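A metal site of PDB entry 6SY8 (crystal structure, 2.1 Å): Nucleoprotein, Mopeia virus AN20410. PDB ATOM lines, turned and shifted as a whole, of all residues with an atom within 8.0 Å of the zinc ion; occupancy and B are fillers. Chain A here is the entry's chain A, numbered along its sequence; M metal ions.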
ATOM      1  N   GLU A  28     -13.253  19.993  -4.290  1.00  0.00           N
ATOM      2  CA  GLU A  28     -13.542  19.010  -3.257  1.00  0.00           C
ATOM      3  C   GLU A  28     -14.713  19.645  -2.434  1.00  0.00           C
ATOM      4  O   GLU A  28     -14.850  20.875  -2.402  1.00  0.00           O
ATOM      5  CB  GLU A  28     -12.326  18.634  -2.396  1.00  0.00           C
ATOM      6  CG  GLU A  28     -11.146  18.036  -3.157  1.00  0.00           C
ATOM      7  CD  GLU A  28     -11.447  16.968  -4.204  1.00  0.00           C
ATOM      8  OE1 GLU A  28     -12.270  16.069  -3.934  1.00  0.00           O
ATOM      9  OE2 GLU A  28     -10.831  17.035  -5.301  1.00  0.00           O
ATOM     10  N   VAL A  35     -14.842  22.928  -0.218  1.00  0.00           N
ATOM     11  CA  VAL A  35     -13.751  23.063   0.766  1.00  0.00           C
ATOM     12  C   VAL A  35     -12.370  23.283   0.117  1.00  0.00           C
ATOM     13  O   VAL A  35     -11.470  23.734   0.807  1.00  0.00           O
ATOM     14  CB  VAL A  35     -13.680  21.944   1.797  1.00  0.00           C
ATOM     15  CG1 VAL A  35     -14.892  21.959   2.715  1.00  0.00           C
ATOM     16  CG2 VAL A  35     -13.477  20.592   1.151  1.00  0.00           C
ATOM     17  N   GLU A  36     -12.197  22.910  -1.170  1.00  0.00           N
ATOM     18  CA  GLU A  36     -10.902  23.065  -1.867  1.00  0.00           C
ATOM     19  C   GLU A  36     -11.149  23.272  -3.347  1.00  0.00           C
ATOM     20  O   GLU A  36     -11.874  22.484  -3.962  1.00  0.00           O
ATOM     21  CB  GLU A  36      -9.994  21.856  -1.600  1.00  0.00           C
ATOM     22  CG  GLU A  36      -8.549  22.026  -2.057  1.00  0.00           C
ATOM     23  CD  GLU A  36      -7.714  20.765  -1.954  1.00  0.00           C
ATOM     24  OE1 GLU A  36      -8.307  19.666  -1.961  1.00  0.00           O
ATOM     25  OE2 GLU A  36      -6.471  20.872  -1.868  1.00  0.00           O
ATOM     26  N   ILE A  37     -10.606  24.342  -3.900  1.00  0.00           N
ATOM     27  CA  ILE A  37     -10.742  24.692  -5.317  1.00  0.00           C
ATOM     28  C   ILE A  37      -9.358  24.874  -5.993  1.00  0.00           C
ATOM     29  O   ILE A  37      -8.467  25.496  -5.412  1.00  0.00           O
ATOM     30  CB  ILE A  37     -11.625  25.939  -5.527  1.00  0.00           C
ATOM     31  CG1 ILE A  37     -13.038  25.741  -4.915  1.00  0.00           C
ATOM     32  CG2 ILE A  37     -11.693  26.381  -6.986  1.00  0.00           C
ATOM     33  CD1 ILE A  37     -13.979  26.946  -5.172  1.00  0.00           C
ATOM     34  N   ALA A  38      -9.202  24.338  -7.237  1.00  0.00           N
ATOM     35  CA  ALA A  38      -7.983  24.452  -8.023  1.00  0.00           C
ATOM     36  C   ALA A  38      -8.279  24.839  -9.473  1.00  0.00           C
ATOM     37  O   ALA A  38      -9.101  24.192 -10.117  1.00  0.00           O
ATOM     38  CB  ALA A  38      -7.188  23.179  -7.936  1.00  0.00           C
ATOM     39  N   HIS A  49      -5.121  27.990  -6.066  1.00  0.00           N
ATOM     40  CA  HIS A  49      -5.450  26.906  -5.164  1.00  0.00           C
ATOM     41  C   HIS A  49      -5.783  27.410  -3.756  1.00  0.00           C
ATOM     42  O   HIS A  49      -4.940  27.983  -3.069  1.00  0.00           O
ATOM     43  CB  HIS A  49      -4.336  25.862  -5.160  1.00  0.00           C
ATOM     44  CG  HIS A  49      -4.554  24.725  -4.232  1.00  0.00           C
ATOM     45  ND1 HIS A  49      -3.531  24.223  -3.455  1.00  0.00           N
ATOM     46  CD2 HIS A  49      -5.672  24.002  -3.990  1.00  0.00           C
ATOM     47  CE1 HIS A  49      -4.045  23.220  -2.778  1.00  0.00           C
ATOM     48  NE2 HIS A  49      -5.337  23.052  -3.046  1.00  0.00           N
ATOM     49  N   PHE A  50      -7.001  27.201  -3.307  1.00  0.00           N
ATOM     50  CA  PHE A  50      -7.413  27.724  -1.992  1.00  0.00           C
ATOM     51  C   PHE A  50      -8.377  26.839  -1.314  1.00  0.00           C
ATOM     52  O   PHE A  50      -8.851  25.890  -1.941  1.00  0.00           O
ATOM     53  CB  PHE A  50      -7.959  29.144  -2.101  1.00  0.00           C
ATOM     54  CG  PHE A  50      -9.131  29.307  -3.041  1.00  0.00           C
ATOM     55  CD1 PHE A  50      -8.940  29.568  -4.391  1.00  0.00           C
ATOM     56  CD2 PHE A  50     -10.437  29.157  -2.580  1.00  0.00           C
ATOM     57  CE1 PHE A  50     -10.031  29.676  -5.264  1.00  0.00           C
ATOM     58  CE2 PHE A  50     -11.523  29.245  -3.463  1.00  0.00           C
ATOM     59  CZ  PHE A  50     -11.315  29.550  -4.779  1.00  0.00           C
ATOM     60  N   TYR A  51      -8.665  27.134  -0.055  1.00  0.00           N
ATOM     61  CA  TYR A  51      -9.555  26.323   0.755  1.00  0.00           C
ATOM     62  C   TYR A  51     -10.765  27.119   1.289  1.00  0.00           C
ATOM     63  O   TYR A  51     -10.848  28.363   1.118  1.00  0.00           O
ATOM     64  CB  TYR A  51      -8.807  25.642   1.902  1.00  0.00           C
ATOM     65  CG  TYR A  51      -7.457  25.104   1.529  1.00  0.00           C
ATOM     66  CD1 TYR A  51      -7.320  23.799   1.047  1.00  0.00           C
ATOM     67  CD2 TYR A  51      -6.306  25.877   1.639  1.00  0.00           C
ATOM     68  CE1 TYR A  51      -6.078  23.300   0.674  1.00  0.00           C
ATOM     69  CE2 TYR A  51      -5.065  25.388   1.287  1.00  0.00           C
ATOM     70  CZ  TYR A  51      -4.952  24.100   0.789  1.00  0.00           C
ATOM     71  OH  TYR A  51      -3.711  23.593   0.450  1.00  0.00           O
ATOM     72  N   HIS A  68     -11.588  13.267   0.833  1.00  0.00           N
ATOM     73  CA  HIS A  68     -10.458  14.187   0.930  1.00  0.00           C
ATOM     74  C   HIS A  68      -9.580  14.092   2.207  1.00  0.00           C
ATOM     75  O   HIS A  68      -8.465  14.614   2.203  1.00  0.00           O
ATOM     76  CB  HIS A  68     -10.921  15.632   0.698  1.00  0.00           C
ATOM     77  CG  HIS A  68     -12.018  16.105   1.610  1.00  0.00           C
ATOM     78  ND1 HIS A  68     -11.867  16.096   3.002  1.00  0.00           N
ATOM     79  CD2 HIS A  68     -13.222  16.652   1.319  1.00  0.00           C
ATOM     80  CE1 HIS A  68     -12.968  16.616   3.492  1.00  0.00           C
ATOM     81  NE2 HIS A  68     -13.826  16.962   2.517  1.00  0.00           N
ATOM     82  N   ILE A  70      -9.520  15.630   4.919  1.00  0.00           N
ATOM     83  CA  ILE A  70      -9.189  16.900   5.575  1.00  0.00           C
ATOM     84  C   ILE A  70      -9.733  16.917   7.009  1.00  0.00           C
ATOM     85  O   ILE A  70     -10.869  16.499   7.246  1.00  0.00           O
ATOM     86  CB  ILE A  70      -9.724  18.081   4.721  1.00  0.00           C
ATOM     87  CG1 ILE A  70      -9.116  18.050   3.298  1.00  0.00           C
ATOM     88  CG2 ILE A  70      -9.468  19.432   5.424  1.00  0.00           C
ATOM     89  CD1 ILE A  70      -9.812  18.960   2.208  1.00  0.00           C
ATOM     90  N   TRP A 136       1.374  11.910  -6.711  1.00  0.00           N
ATOM     91  CA  TRP A 136       1.472  12.069  -5.269  1.00  0.00           C
ATOM     92  C   TRP A 136       2.939  12.020  -4.821  1.00  0.00           C
ATOM     93  O   TRP A 136       3.331  12.820  -3.977  1.00  0.00           O
ATOM     94  CB  TRP A 136       0.581  11.077  -4.490  1.00  0.00           C
ATOM     95  CG  TRP A 136      -0.838  11.571  -4.284  1.00  0.00           C
ATOM     96  CD1 TRP A 136      -1.846  11.569  -5.204  1.00  0.00           C
ATOM     97  CD2 TRP A 136      -1.367  12.216  -3.110  1.00  0.00           C
ATOM     98  NE1 TRP A 136      -2.972  12.158  -4.669  1.00  0.00           N
ATOM     99  CE2 TRP A 136      -2.696  12.584  -3.401  1.00  0.00           C
ATOM    100  CE3 TRP A 136      -0.830  12.561  -1.853  1.00  0.00           C
ATOM    101  CZ2 TRP A 136      -3.506  13.284  -2.479  1.00  0.00           C
ATOM    102  CZ3 TRP A 136      -1.639  13.220  -0.940  1.00  0.00           C
ATOM    103  CH2 TRP A 136      -2.962  13.573  -1.258  1.00  0.00           C
ATOM    104  N   LYS A 140       3.257  15.834  -3.544  1.00  0.00           N
ATOM    105  CA  LYS A 140       2.631  15.756  -2.218  1.00  0.00           C
ATOM    106  C   LYS A 140       2.869  17.036  -1.402  1.00  0.00           C
ATOM    107  O   LYS A 140       1.966  17.483  -0.686  1.00  0.00           O
ATOM    108  CB  LYS A 140       3.208  14.599  -1.398  1.00  0.00           C
ATOM    109  CG  LYS A 140       2.149  13.629  -0.928  1.00  0.00           C
ATOM    110  CD  LYS A 140       2.586  12.718   0.207  1.00  0.00           C
ATOM    111  CE  LYS A 140       1.393  11.979   0.780  1.00  0.00           C
ATOM    112  NZ  LYS A 140       1.774  11.114   1.930  1.00  0.00           N
ATOM    113  N   LEU A 142       3.023  20.035  -2.283  1.00  0.00           N
ATOM    114  CA  LEU A 142       2.182  21.152  -2.706  1.00  0.00           C
ATOM    115  C   LEU A 142       0.873  21.282  -1.924  1.00  0.00           C
ATOM    116  O   LEU A 142       0.229  22.342  -2.034  1.00  0.00           O
ATOM    117  CB  LEU A 142       1.897  21.152  -4.206  1.00  0.00           C
ATOM    118  CG  LEU A 142       3.054  21.270  -5.177  1.00  0.00           C
ATOM    119  CD1 LEU A 142       2.542  21.175  -6.625  1.00  0.00           C
ATOM    120  CD2 LEU A 142       3.788  22.602  -5.015  1.00  0.00           C
ATOM    121  N   CYS A 143       0.451  20.240  -1.159  1.00  0.00           N
ATOM    122  CA  CYS A 143      -0.762  20.275  -0.355  1.00  0.00           C
ATOM    123  C   CYS A 143      -0.708  19.250   0.734  1.00  0.00           C
ATOM    124  O   CYS A 143      -0.825  18.048   0.475  1.00  0.00           O
ATOM    125  CB  CYS A 143      -2.036  20.176  -1.187  1.00  0.00           C
ATOM    126  SG  CYS A 143      -3.552  20.591  -0.262  1.00  0.00           S
ATOM    127  N   ARG A 144      -0.551  19.725   1.986  1.00  0.00           N
ATOM    128  CA  ARG A 144      -0.462  18.861   3.173  1.00  0.00           C
ATOM    129  C   ARG A 144      -1.774  18.842   3.967  1.00  0.00           C
ATOM    130  O   ARG A 144      -1.777  18.453   5.127  1.00  0.00           O
ATOM    131  CB  ARG A 144       0.733  19.290   4.070  1.00  0.00           C
ATOM    132  CG  ARG A 144       2.106  18.854   3.550  1.00  0.00           C
ATOM    133  CD  ARG A 144       3.177  18.841   4.634  1.00  0.00           C
ATOM    134  NE  ARG A 144       3.899  20.128   4.738  1.00  0.00           N
ATOM    135  CZ  ARG A 144       3.888  20.913   5.815  1.00  0.00           C
ATOM    136  NH1 ARG A 144       3.212  20.561   6.907  1.00  0.00           N
ATOM    137  NH2 ARG A 144       4.553  22.061   5.818  1.00  0.00           N
ATOM    138  N   MET A 145      -2.873  19.251   3.326  1.00  0.00           N
ATOM    139  CA  MET A 145      -4.179  19.364   3.967  1.00  0.00           C
ATOM    140  C   MET A 145      -4.940  18.050   4.129  1.00  0.00           C
ATOM    141  O   MET A 145      -5.902  18.022   4.873  1.00  0.00           O
ATOM    142  CB  MET A 145      -5.028  20.370   3.215  1.00  0.00           C
ATOM    143  CG  MET A 145      -4.486  21.770   3.328  1.00  0.00           C
ATOM    144  SD  MET A 145      -4.826  22.619   4.907  1.00  0.00           S
ATOM    145  CE  MET A 145      -6.470  22.154   5.192  1.00  0.00           C
ATOM    146  N   HIS A 146      -4.495  16.968   3.460  1.00  0.00           N
ATOM    147  CA  HIS A 146      -5.155  15.657   3.471  1.00  0.00           C
ATOM    148  C   HIS A 146      -4.447  14.687   4.417  1.00  0.00           C
ATOM    149  O   HIS A 146      -3.634  13.877   3.992  1.00  0.00           O
ATOM    150  CB  HIS A 146      -5.232  15.138   2.021  1.00  0.00           C
ATOM    151  CG  HIS A 146      -5.611  16.197   1.037  1.00  0.00           C
ATOM    152  ND1 HIS A 146      -6.947  16.460   0.721  1.00  0.00           N
ATOM    153  CD2 HIS A 146      -4.824  17.091   0.379  1.00  0.00           C
ATOM    154  CE1 HIS A 146      -6.917  17.483  -0.128  1.00  0.00           C
ATOM    155  NE2 HIS A 146      -5.661  17.938  -0.316  1.00  0.00           N
ATOM    156  N   PRO A 164      -6.017   9.992  -0.632  1.00  0.00           N
ATOM    157  CA  PRO A 164      -6.997  11.076  -0.539  1.00  0.00           C
ATOM    158  C   PRO A 164      -7.073  11.891  -1.821  1.00  0.00           C
ATOM    159  O   PRO A 164      -6.125  11.943  -2.607  1.00  0.00           O
ATOM    160  CB  PRO A 164      -6.486  11.930   0.625  1.00  0.00           C
ATOM    161  CG  PRO A 164      -5.580  11.033   1.387  1.00  0.00           C
ATOM    162  CD  PRO A 164      -4.940  10.175   0.362  1.00  0.00           C
ATOM    163  N   HIS A 165      -8.225  12.524  -2.031  1.00  0.00           N
ATOM    164  CA  HIS A 165      -8.469  13.335  -3.206  1.00  0.00           C
ATOM    165  C   HIS A 165      -8.150  14.797  -2.902  1.00  0.00           C
ATOM    166  O   HIS A 165      -8.639  15.354  -1.932  1.00  0.00           O
ATOM    167  CB  HIS A 165      -9.933  13.176  -3.662  1.00  0.00           C
ATOM    168  CG  HIS A 165     -10.259  11.825  -4.254  1.00  0.00           C
ATOM    169  ND1 HIS A 165     -11.433  11.623  -4.971  1.00  0.00           N
ATOM    170  CD2 HIS A 165      -9.572  10.662  -4.221  1.00  0.00           C
ATOM    171  CE1 HIS A 165     -11.407  10.360  -5.347  1.00  0.00           C
ATOM    172  NE2 HIS A 165     -10.309   9.738  -4.911  1.00  0.00           N
ATOM    173  N   CYS A 166      -7.301  15.392  -3.729  1.00  0.00           N
ATOM    174  CA  CYS A 166      -6.875  16.765  -3.585  1.00  0.00           C
ATOM    175  C   CYS A 166      -7.271  17.498  -4.856  1.00  0.00           C
ATOM    176  O   CYS A 166      -6.953  17.032  -5.935  1.00  0.00           O
ATOM    177  CB  CYS A 166      -5.368  16.841  -3.320  1.00  0.00           C
ATOM    178  SG  CYS A 166      -4.633  18.501  -3.537  1.00  0.00           S
ATOM    179  N   ALA A 167      -7.976  18.650  -4.750  1.00  0.00           N
ATOM    180  CA  ALA A 167      -8.381  19.413  -5.936  1.00  0.00           C
ATOM    181  C   ALA A 167      -7.217  19.705  -6.836  1.00  0.00           C
ATOM    182  O   ALA A 167      -7.360  19.654  -8.065  1.00  0.00           O
ATOM    183  CB  ALA A 167      -9.059  20.722  -5.536  1.00  0.00           C
ATOM    184  N   LEU A 168      -6.068  20.066  -6.243  1.00  0.00           N
ATOM    185  CA  LEU A 168      -4.871  20.406  -6.976  1.00  0.00           C
ATOM    186  C   LEU A 168      -4.266  19.227  -7.692  1.00  0.00           C
ATOM    187  O   LEU A 168      -4.031  19.313  -8.881  1.00  0.00           O
ATOM    188  CB  LEU A 168      -3.815  21.075  -6.069  1.00  0.00           C
ATOM    189  CG  LEU A 168      -2.504  21.476  -6.761  1.00  0.00           C
ATOM    190  CD1 LEU A 168      -2.748  22.455  -7.938  1.00  0.00           C
ATOM    191  CD2 LEU A 168      -1.510  22.021  -5.743  1.00  0.00           C
ATOM    192  N   LEU A 169      -3.967  18.151  -6.957  1.00  0.00           N
ATOM    193  CA  LEU A 169      -3.292  16.997  -7.493  1.00  0.00           C
ATOM    194  C   LEU A 169      -4.142  16.303  -8.529  1.00  0.00           C
ATOM    195  O   LEU A 169      -3.609  15.820  -9.528  1.00  0.00           O
ATOM    196  CB  LEU A 169      -2.797  16.064  -6.373  1.00  0.00           C
ATOM    197  CG  LEU A 169      -1.304  16.259  -5.968  1.00  0.00           C
ATOM    198  CD1 LEU A 169      -1.014  17.692  -5.547  1.00  0.00           C
ATOM    199  CD2 LEU A 169      -0.913  15.333  -4.808  1.00  0.00           C
ATOM    200  N   ASP A 170      -5.475  16.366  -8.364  1.00  0.00           N
ATOM    201  CA  ASP A 170      -6.431  15.822  -9.315  1.00  0.00           C
ATOM    202  C   ASP A 170      -6.278  16.538 -10.600  1.00  0.00           C
ATOM    203  O   ASP A 170      -6.225  15.856 -11.615  1.00  0.00           O
ATOM    204  CB  ASP A 170      -7.874  15.907  -8.798  1.00  0.00           C
ATOM    205  CG  ASP A 170      -8.196  14.833  -7.787  1.00  0.00           C
ATOM    206  OD1 ASP A 170      -7.283  14.079  -7.412  1.00  0.00           O
ATOM    207  OD2 ASP A 170      -9.363  14.760  -7.381  1.00  0.00           O
HETATM  208 ZN    ZN M   1      -5.319  19.395  -1.437  1.00  0.00          ZN
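ND1 of His 146 lies close to O of His 165 (3.3 Å).
A ring nitrogen (ND1) of His 146 sits at hydrogen-bond distance from the backbone carbonyl oxygen (O) of His 68.
The backbone NH (N) of Ala 167 is in hydrogen-bond range of the side-chain carboxylate (OE1) of Glu 36.
O of Glu 36 sits at hydrogen-bond distance from N of Glu 28 (2.9 Å).
The side-chain sulfur (SG) of Cys 143 sits close to the side-chain hydroxyl (OH) of Tyr 51, at 3.1 Å.
The side-chain sulfur (SG) of Cys 166 sits close to the backbone NH (N) of Leu 168, 3.4 Å away.
The side-chain carboxylate (OE2) of Glu 36 sits close to a ring nitrogen (NE2) of His 49, 2.7 Å away.
The side-chain sulfur of Cys 166 lies close to the backbone NH of Leu 169, 3.5 Å away.
His 49 touches the zinc ion.
Five residues have an atom within 4 Å of the zinc ion: Glu 36, His 49, Cys 143, His 146 and Cys 166.
Along chain A the residues within 4 Å of the zinc ion span positions 36 to 166.
The nearest printed residue that does not touch the zinc ion is Ala 167 (4.3 Å).
The zinc ion is bound by a ring nitrogen (NE2) of His 146, the side-chain carboxylate of Glu 36, the side-chain sulfur of Cys 166 and the side-chain sulfur of Cys 143.
The zinc ion has four donor atoms within binding distance.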
